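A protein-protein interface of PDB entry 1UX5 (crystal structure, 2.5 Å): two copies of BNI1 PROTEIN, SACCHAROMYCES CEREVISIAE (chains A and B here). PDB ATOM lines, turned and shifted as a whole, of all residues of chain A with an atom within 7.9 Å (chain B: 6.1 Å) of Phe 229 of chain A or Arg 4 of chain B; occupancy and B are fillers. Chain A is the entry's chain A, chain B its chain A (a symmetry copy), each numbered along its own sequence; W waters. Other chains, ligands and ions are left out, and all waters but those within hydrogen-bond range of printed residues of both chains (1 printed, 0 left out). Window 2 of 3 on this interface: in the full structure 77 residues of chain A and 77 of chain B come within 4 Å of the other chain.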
ATOM      1  N   VAL A 222      20.348  13.002  17.570  1.00  0.00           N
ATOM      2  CA  VAL A 222      20.801  11.809  16.895  1.00  0.00           C
ATOM      3  C   VAL A 222      19.567  10.910  16.827  1.00  0.00           C
ATOM      4  O   VAL A 222      19.234  10.371  15.764  1.00  0.00           O
ATOM      5  CB  VAL A 222      21.924  11.131  17.686  1.00  0.00           C
ATOM      6  CG1 VAL A 222      22.220   9.765  17.103  1.00  0.00           C
ATOM      7  CG2 VAL A 222      23.176  12.003  17.635  1.00  0.00           C
ATOM      8  N   ILE A 223      18.869  10.776  17.954  1.00  0.00           N
ATOM      9  CA  ILE A 223      17.662   9.954  17.982  1.00  0.00           C
ATOM     10  C   ILE A 223      16.670  10.479  16.952  1.00  0.00           C
ATOM     11  O   ILE A 223      16.010   9.698  16.259  1.00  0.00           O
ATOM     12  CB  ILE A 223      16.971   9.979  19.352  1.00  0.00           C
ATOM     13  CG1 ILE A 223      17.880   9.328  20.399  1.00  0.00           C
ATOM     14  CG2 ILE A 223      15.610   9.281  19.265  1.00  0.00           C
ATOM     15  CD1 ILE A 223      17.285   9.325  21.794  1.00  0.00           C
ATOM     16  N   LEU A 224      16.563  11.800  16.844  1.00  0.00           N
ATOM     17  CA  LEU A 224      15.626  12.362  15.883  1.00  0.00           C
ATOM     18  C   LEU A 224      16.051  12.045  14.452  1.00  0.00           C
ATOM     19  O   LEU A 224      15.224  11.658  13.626  1.00  0.00           O
ATOM     20  CB  LEU A 224      15.511  13.871  16.048  1.00  0.00           C
ATOM     21  CG  LEU A 224      14.385  14.396  15.160  1.00  0.00           C
ATOM     22  CD1 LEU A 224      13.079  13.815  15.645  1.00  0.00           C
ATOM     23  CD2 LEU A 224      14.320  15.893  15.189  1.00  0.00           C
ATOM     24  N   ALA A 225      17.340  12.209  14.164  1.00  0.00           N
ATOM     25  CA  ALA A 225      17.853  11.938  12.828  1.00  0.00           C
ATOM     26  C   ALA A 225      17.459  10.533  12.420  1.00  0.00           C
ATOM     27  O   ALA A 225      16.707  10.345  11.461  1.00  0.00           O
ATOM     28  CB  ALA A 225      19.358  12.084  12.800  1.00  0.00           C
ATOM     29  N   VAL A 226      17.977   9.556  13.159  1.00  0.00           N
ATOM     30  CA  VAL A 226      17.694   8.143  12.918  1.00  0.00           C
ATOM     31  C   VAL A 226      16.185   7.919  12.810  1.00  0.00           C
ATOM     32  O   VAL A 226      15.691   7.310  11.851  1.00  0.00           O
ATOM     33  CB  VAL A 226      18.234   7.271  14.074  1.00  0.00           C
ATOM     34  CG1 VAL A 226      17.756   5.850  13.925  1.00  0.00           C
ATOM     35  CG2 VAL A 226      19.740   7.312  14.086  1.00  0.00           C
ATOM     36  N   GLY A 227      15.461   8.419  13.804  1.00  0.00           N
ATOM     37  CA  GLY A 227      14.021   8.280  13.802  1.00  0.00           C
ATOM     38  C   GLY A 227      13.394   8.711  12.488  1.00  0.00           C
ATOM     39  O   GLY A 227      12.605   7.967  11.906  1.00  0.00           O
ATOM     40  N   ASN A 228      13.737   9.904  12.005  1.00  0.00           N
ATOM     41  CA  ASN A 228      13.156  10.373  10.751  1.00  0.00           C
ATOM     42  C   ASN A 228      13.590   9.510   9.584  1.00  0.00           C
ATOM     43  O   ASN A 228      12.853   9.330   8.620  1.00  0.00           O
ATOM     44  CB  ASN A 228      13.524  11.831  10.464  1.00  0.00           C
ATOM     45  CG  ASN A 228      12.682  12.818  11.261  1.00  0.00           C
ATOM     46  OD1 ASN A 228      11.467  12.638  11.426  1.00  0.00           O
ATOM     47  ND2 ASN A 228      13.320  13.880  11.740  1.00  0.00           N
ATOM     48  N   PHE A 229      14.795   8.970   9.673  1.00  0.00           N
ATOM     49  CA  PHE A 229      15.295   8.133   8.603  1.00  0.00           C
ATOM     50  C   PHE A 229      14.426   6.891   8.462  1.00  0.00           C
ATOM     51  O   PHE A 229      14.107   6.474   7.355  1.00  0.00           O
ATOM     52  CB  PHE A 229      16.718   7.721   8.903  1.00  0.00           C
ATOM     53  CG  PHE A 229      17.278   6.769   7.917  1.00  0.00           C
ATOM     54  CD1 PHE A 229      17.598   7.190   6.633  1.00  0.00           C
ATOM     55  CD2 PHE A 229      17.495   5.444   8.269  1.00  0.00           C
ATOM     56  CE1 PHE A 229      18.137   6.302   5.699  1.00  0.00           C
ATOM     57  CE2 PHE A 229      18.031   4.547   7.351  1.00  0.00           C
ATOM     58  CZ  PHE A 229      18.355   4.978   6.059  1.00  0.00           C
ATOM     59  N   MET A 230      14.023   6.311   9.584  1.00  0.00           N
ATOM     60  CA  MET A 230      13.206   5.103   9.546  1.00  0.00           C
ATOM     61  C   MET A 230      11.735   5.331   9.228  1.00  0.00           C
ATOM     62  O   MET A 230      11.139   4.586   8.450  1.00  0.00           O
ATOM     63  CB  MET A 230      13.287   4.370  10.875  1.00  0.00           C
ATOM     64  CG  MET A 230      14.672   4.055  11.321  1.00  0.00           C
ATOM     65  SD  MET A 230      14.537   3.510  13.014  1.00  0.00           S
ATOM     66  CE  MET A 230      15.187   1.840  12.858  1.00  0.00           C
ATOM     67  N   ASN A 231      11.145   6.344   9.846  1.00  0.00           N
ATOM     68  CA  ASN A 231       9.735   6.617   9.628  1.00  0.00           C
ATOM     69  C   ASN A 231       9.333   7.069   8.230  1.00  0.00           C
ATOM     70  O   ASN A 231      10.119   7.670   7.491  1.00  0.00           O
ATOM     71  CB  ASN A 231       9.246   7.653  10.636  1.00  0.00           C
ATOM     72  CG  ASN A 231       9.190   7.109  12.038  1.00  0.00           C
ATOM     73  OD1 ASN A 231       9.280   5.897  12.246  1.00  0.00           O
ATOM     74  ND2 ASN A 231       9.025   7.996  13.012  1.00  0.00           N
ATOM     75  N   ASP A 232       8.092   6.755   7.875  1.00  0.00           N
ATOM     76  CA  ASP A 232       7.535   7.157   6.598  1.00  0.00           C
ATOM     77  C   ASP A 232       7.202   8.641   6.747  1.00  0.00           C
ATOM     78  O   ASP A 232       7.413   9.219   7.820  1.00  0.00           O
ATOM     79  CB  ASP A 232       6.288   6.333   6.281  1.00  0.00           C
ATOM     80  CG  ASP A 232       5.263   6.367   7.394  1.00  0.00           C
ATOM     81  OD1 ASP A 232       4.571   5.340   7.590  1.00  0.00           O
ATOM     82  OD2 ASP A 232       5.139   7.418   8.060  1.00  0.00           O
ATOM     83  N   THR A 233       6.676   9.264   5.698  1.00  0.00           N
ATOM     84  CA  THR A 233       6.396  10.696   5.768  1.00  0.00           C
ATOM     85  C   THR A 233       5.328  11.103   6.774  1.00  0.00           C
ATOM     86  O   THR A 233       5.391  12.197   7.340  1.00  0.00           O
ATOM     87  CB  THR A 233       6.030  11.267   4.373  1.00  0.00           C
ATOM     88  OG1 THR A 233       4.905  10.561   3.848  1.00  0.00           O
ATOM     89  CG2 THR A 233       7.210  11.128   3.407  1.00  0.00           C
ATOM     90  N   LYS A 235       4.957  10.089   9.672  1.00  0.00           N
ATOM     91  CA  LYS A 235       5.560  10.186  10.994  1.00  0.00           C
ATOM     92  C   LYS A 235       6.788  11.083  11.077  1.00  0.00           C
ATOM     93  O   LYS A 235       7.464  11.108  12.118  1.00  0.00           O
ATOM     94  CB  LYS A 235       5.931   8.794  11.523  1.00  0.00           C
ATOM     95  CG  LYS A 235       4.754   7.849  11.681  1.00  0.00           C
ATOM     96  CD  LYS A 235       5.206   6.532  12.286  1.00  0.00           C
ATOM     97  CE  LYS A 235       4.246   5.412  11.942  1.00  0.00           C
ATOM     98  NZ  LYS A 235       4.185   5.143  10.470  1.00  0.00           N
ATOM     99  N   GLN A 236       7.105  11.809  10.008  1.00  0.00           N
ATOM    100  CA  GLN A 236       8.267  12.693  10.083  1.00  0.00           C
ATOM    101  C   GLN A 236       8.005  13.734  11.175  1.00  0.00           C
ATOM    102  O   GLN A 236       6.871  14.199  11.353  1.00  0.00           O
ATOM    103  CB  GLN A 236       8.515  13.392   8.745  1.00  0.00           C
ATOM    104  CG  GLN A 236       8.941  12.458   7.617  1.00  0.00           C
ATOM    105  CD  GLN A 236      10.186  11.671   7.961  1.00  0.00           C
ATOM    106  OE1 GLN A 236      11.263  12.235   8.161  1.00  0.00           O
ATOM    107  NE2 GLN A 236      10.045  10.355   8.037  1.00  0.00           N
ATOM    108  N   ALA A 237       9.049  14.101  11.912  1.00  0.00           N
ATOM    109  CA  ALA A 237       8.882  15.070  12.983  1.00  0.00           C
ATOM    110  C   ALA A 237      10.024  16.062  13.144  1.00  0.00           C
ATOM    111  O   ALA A 237      11.185  15.756  12.852  1.00  0.00           O
ATOM    112  CB  ALA A 237       8.652  14.347  14.297  1.00  0.00           C
ATOM    113  N   LYS B   1      15.135  15.795   0.802  1.00  0.00           N
ATOM    114  CA  LYS B   1      16.074  16.599   1.650  1.00  0.00           C
ATOM    115  C   LYS B   1      16.366  15.915   2.990  1.00  0.00           C
ATOM    116  O   LYS B   1      16.247  16.531   4.053  1.00  0.00           O
ATOM    117  CB  LYS B   1      15.488  17.994   1.906  1.00  0.00           C
ATOM    118  CG  LYS B   1      15.305  18.837   0.651  1.00  0.00           C
ATOM    119  CD  LYS B   1      14.837  20.250   0.987  1.00  0.00           C
ATOM    120  CE  LYS B   1      14.750  21.120  -0.265  1.00  0.00           C
ATOM    121  NZ  LYS B   1      14.363  22.530   0.030  1.00  0.00           N
ATOM    122  N   TYR B   2      16.758  14.646   2.926  1.00  0.00           N
ATOM    123  CA  TYR B   2      17.059  13.839   4.112  1.00  0.00           C
ATOM    124  C   TYR B   2      17.417  12.491   3.520  1.00  0.00           C
ATOM    125  O   TYR B   2      16.810  12.068   2.529  1.00  0.00           O
ATOM    126  CB  TYR B   2      15.806  13.637   4.972  1.00  0.00           C
ATOM    127  CG  TYR B   2      15.920  13.951   6.461  1.00  0.00           C
ATOM    128  CD1 TYR B   2      15.343  15.112   6.985  1.00  0.00           C
ATOM    129  CD2 TYR B   2      16.547  13.066   7.354  1.00  0.00           C
ATOM    130  CE1 TYR B   2      15.374  15.393   8.349  1.00  0.00           C
ATOM    131  CE2 TYR B   2      16.590  13.343   8.739  1.00  0.00           C
ATOM    132  CZ  TYR B   2      15.993  14.514   9.224  1.00  0.00           C
ATOM    133  OH  TYR B   2      15.991  14.829  10.571  1.00  0.00           O
ATOM    134  N   PRO B   3      18.408  11.797   4.095  1.00  0.00           N
ATOM    135  CA  PRO B   3      18.704  10.497   3.485  1.00  0.00           C
ATOM    136  C   PRO B   3      17.465   9.627   3.632  1.00  0.00           C
ATOM    137  O   PRO B   3      16.718   9.770   4.601  1.00  0.00           O
ATOM    138  CB  PRO B   3      19.873   9.980   4.312  1.00  0.00           C
ATOM    139  CG  PRO B   3      20.579  11.248   4.719  1.00  0.00           C
ATOM    140  CD  PRO B   3      19.425  12.165   5.096  1.00  0.00           C
ATOM    141  N   ARG B   4      17.228   8.749   2.664  1.00  0.00           N
ATOM    142  CA  ARG B   4      16.070   7.870   2.724  1.00  0.00           C
ATOM    143  C   ARG B   4      16.439   6.444   2.411  1.00  0.00           C
ATOM    144  O   ARG B   4      17.288   6.161   1.553  1.00  0.00           O
ATOM    145  CB  ARG B   4      14.981   8.350   1.773  1.00  0.00           C
ATOM    146  CG  ARG B   4      14.393   9.680   2.198  1.00  0.00           C
ATOM    147  CD  ARG B   4      13.768   9.544   3.570  1.00  0.00           C
ATOM    148  NE  ARG B   4      13.504  10.824   4.217  1.00  0.00           N
ATOM    149  CZ  ARG B   4      12.821  10.942   5.352  1.00  0.00           C
ATOM    150  NH1 ARG B   4      12.330   9.856   5.954  1.00  0.00           N
ATOM    151  NH2 ARG B   4      12.642  12.139   5.897  1.00  0.00           N
ATOM    152  N   PRO B   5      15.809   5.511   3.113  1.00  0.00           N
ATOM    153  CA  PRO B   5      16.096   4.094   2.893  1.00  0.00           C
ATOM    154  C   PRO B   5      15.448   3.577   1.612  1.00  0.00           C
ATOM    155  O   PRO B   5      14.395   4.065   1.195  1.00  0.00           O
ATOM    156  CB  PRO B   5      15.536   3.439   4.153  1.00  0.00           C
ATOM    157  CG  PRO B   5      14.314   4.297   4.439  1.00  0.00           C
ATOM    158  CD  PRO B   5      14.816   5.708   4.184  1.00  0.00           C
ATOM    159  N   HIS B   6      16.092   2.598   0.986  1.00  0.00           N
ATOM    160  CA  HIS B   6      15.572   2.000  -0.233  1.00  0.00           C
ATOM    161  C   HIS B   6      14.531   0.939   0.129  1.00  0.00           C
ATOM    162  O   HIS B   6      13.511   0.810  -0.547  1.00  0.00           O
ATOM    163  CB  HIS B   6      16.700   1.373  -1.052  1.00  0.00           C
ATOM    164  CG  HIS B   6      16.232   0.765  -2.337  1.00  0.00           C
ATOM    165  ND1 HIS B   6      16.418  -0.566  -2.644  1.00  0.00           N
ATOM    166  CD2 HIS B   6      15.544   1.300  -3.374  1.00  0.00           C
ATOM    167  CE1 HIS B   6      15.864  -0.827  -3.813  1.00  0.00           C
ATOM    168  NE2 HIS B   6      15.326   0.288  -4.278  1.00  0.00           N
ATOM    169  N   LEU B   9      11.608   0.341   6.472  1.00  0.00           N
ATOM    170  CA  LEU B   9      12.116  -0.021   7.792  1.00  0.00           C
ATOM    171  C   LEU B   9      11.060  -0.017   8.897  1.00  0.00           C
ATOM    172  O   LEU B   9       9.948   0.500   8.726  1.00  0.00           O
ATOM    173  CB  LEU B   9      13.233   0.948   8.195  1.00  0.00           C
ATOM    174  CG  LEU B   9      14.363   1.217   7.198  1.00  0.00           C
ATOM    175  CD1 LEU B   9      15.259   2.320   7.728  1.00  0.00           C
ATOM    176  CD2 LEU B   9      15.167  -0.046   6.984  1.00  0.00           C
ATOM    177  N   TYR B  38      24.853   9.225   7.298  1.00  0.00           N
ATOM    178  CA  TYR B  38      24.728   8.655   5.978  1.00  0.00           C
ATOM    179  C   TYR B  38      26.092   8.495   5.316  1.00  0.00           C
ATOM    180  O   TYR B  38      26.400   7.415   4.814  1.00  0.00           O
ATOM    181  CB  TYR B  38      23.839   9.516   5.090  1.00  0.00           C
ATOM    182  CG  TYR B  38      23.689   8.965   3.687  1.00  0.00           C
ATOM    183  CD1 TYR B  38      22.609   8.145   3.351  1.00  0.00           C
ATOM    184  CD2 TYR B  38      24.608   9.295   2.681  1.00  0.00           C
ATOM    185  CE1 TYR B  38      22.434   7.671   2.044  1.00  0.00           C
ATOM    186  CE2 TYR B  38      24.446   8.829   1.362  1.00  0.00           C
ATOM    187  CZ  TYR B  38      23.356   8.018   1.055  1.00  0.00           C
ATOM    188  OH  TYR B  38      23.192   7.544  -0.230  1.00  0.00           O
ATOM    189  N   LEU B  43      23.860   4.815   8.384  1.00  0.00           N
ATOM    190  CA  LEU B  43      22.482   4.666   7.948  1.00  0.00           C
ATOM    191  C   LEU B  43      22.278   3.364   7.156  1.00  0.00           C
ATOM    192  O   LEU B  43      21.241   2.711   7.267  1.00  0.00           O
ATOM    193  CB  LEU B  43      22.052   5.876   7.116  1.00  0.00           C
ATOM    194  CG  LEU B  43      21.981   7.204   7.877  1.00  0.00           C
ATOM    195  CD1 LEU B  43      21.138   8.203   7.085  1.00  0.00           C
ATOM    196  CD2 LEU B  43      21.345   6.977   9.243  1.00  0.00           C
ATOM    197  N   ALA B  44      23.271   2.970   6.371  1.00  0.00           N
ATOM    198  CA  ALA B  44      23.146   1.742   5.594  1.00  0.00           C
ATOM    199  C   ALA B  44      23.075   0.521   6.502  1.00  0.00           C
ATOM    200  O   ALA B  44      22.348  -0.433   6.206  1.00  0.00           O
ATOM    201  CB  ALA B  44      24.305   1.611   4.631  1.00  0.00           C
ATOM    202  N   LEU B  46      21.921   0.535   9.562  1.00  0.00           N
ATOM    203  CA  LEU B  46      20.605   0.654  10.163  1.00  0.00           C
ATOM    204  C   LEU B  46      19.544   0.090   9.242  1.00  0.00           C
ATOM    205  O   LEU B  46      18.574  -0.530   9.689  1.00  0.00           O
ATOM    206  CB  LEU B  46      20.289   2.113  10.425  1.00  0.00           C
ATOM    207  CG  LEU B  46      19.864   2.437  11.845  1.00  0.00           C
ATOM    208  CD1 LEU B  46      21.077   2.363  12.767  1.00  0.00           C
ATOM    209  CD2 LEU B  46      19.268   3.819  11.872  1.00  0.00           C
ATOM    210  N   GLU B  47      19.742   0.326   7.949  1.00  0.00           N
ATOM    211  CA  GLU B  47      18.812  -0.114   6.929  1.00  0.00           C
ATOM    212  C   GLU B  47      18.700  -1.624   6.891  1.00  0.00           C
ATOM    213  O   GLU B  47      17.644  -2.175   6.579  1.00  0.00           O
ATOM    214  CB  GLU B  47      19.252   0.405   5.571  1.00  0.00           C
ATOM    215  CG  GLU B  47      18.185   0.282   4.513  1.00  0.00           C
ATOM    216  CD  GLU B  47      18.477   1.146   3.311  1.00  0.00           C
ATOM    217  OE1 GLU B  47      17.694   1.083   2.343  1.00  0.00           O
ATOM    218  OE2 GLU B  47      19.488   1.887   3.338  1.00  0.00           O
HETATM  219  O   HOH W   1      11.210   2.924   6.326  1.00  0.00           O
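O of Asn 231 of chain A lies within hydrogen-bond range of NH1 of Arg 4 of chain B (3.5 Å). OE1 of Gln 236 of chain A sits at hydrogen-bond distance from NH2 of Arg 4 of chain B, at 2.7 Å. The backbone carbonyl oxygen (O) of Asn 228 of chain A is in hydrogen-bond range of the guanidinium group (NH1) of Arg 4 of chain B (2.8 Å). The side-chain hydroxyl (OH) of Tyr 2 of chain B sits at hydrogen-bond distance from the side-chain amide nitrogen (ND2) of Asn 228 of chain A (3.1 Å).
Printed residues of chain B that touch a printed residue of chain A: Tyr 2, Pro 3, Arg 4, Pro 5, Leu 9, Leu 43 and Leu 46. Hydrophobic or aromatic side chains of chain A that line the printed part of chain B: Val 226 and Phe 229. Among the printed residues, no Asp or Glu carboxylate lies within 4 Å of a Lys or Arg side-chain nitrogen of the other chain.
O of Asn 231 of chain A sits at hydrogen-bond distance from NE2 of Gln 236 of chain A (2.7 Å). The backbone carbonyl oxygen of Asn 228 of chain A sits at hydrogen-bond distance from the side-chain amide nitrogen of Gln 236 of chain A, 3.0 Å away. The backbone carbonyl oxygen (O) of Asp 232 of chain A is in hydrogen-bond range of the side-chain amide nitrogen (NE2) of Gln 236 of chain A. The side-chain amide oxygen (OD1) of Asn 228 of chain A sits at hydrogen-bond distance from the backbone NH (N) of Ala 237 of chain A, at 2.9 Å. The backbone carbonyl oxygen (O) of Leu 224 of chain A lies within hydrogen-bond range of the side-chain amide nitrogen (ND2) of Asn 228 of chain A, at 3.5 Å.
Val 222 of chain A touches none of the printed residues of chain B. Gly 227 of chain A touches none of the printed residues of chain B. Phe 229 of chain A touches just these residues of chain B: Pro 3, Arg 4, Pro 5, Leu 9 and Leu 43. Printed residues of chain B within 4 Å of Gln 236 of chain A: Arg 4 (2.7 Å). Arg 4 of chain B touches just these residues of chain A: Asn 228 (2.8 Å), Phe 229 (3.7 Å), Asn 231 (3.5 Å) and Gln 236 (2.7 Å). Pro 5 of chain B touches just one residue of chain A: Phe 229. Of the printed residues of chain A, Leu 9 of chain B touches Phe 229 and Met 230. The nearest residue of chain A that does not touch Arg 4 of chain B is Asp 232 of chain A (5.3 Å).
No position is printed for both chains. Of the 11 pairs that touch across the chains among the printed residues, none has its exchanged pair printed and touching as well.
Water W1 lies within hydrogen-bond range of the backbone NH (N) of Leu 9 of chain B (2.6 Å) and the backbone carbonyl oxygen (O) of Met 230 of chain A (2.7 Å).
Val 226 of chain A touches Leu 46 of chain B (CG1 to CD2, 3.3 Å). CD1 of Phe 229 of chain A touches O of Pro 3 of chain B (3.4 Å). Arg 4 of chain B touches Phe 229 of chain A. O of Phe 229 of chain A touches CD of Pro 5 of chain B (3.3 Å). Phe 229 of chain A touches Leu 9 of chain B (CE2 to CD1, 3.6 Å). Phe 229 of chain A touches Leu 43 of chain B. Leu 9 of chain B touches Met 230 of chain A.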
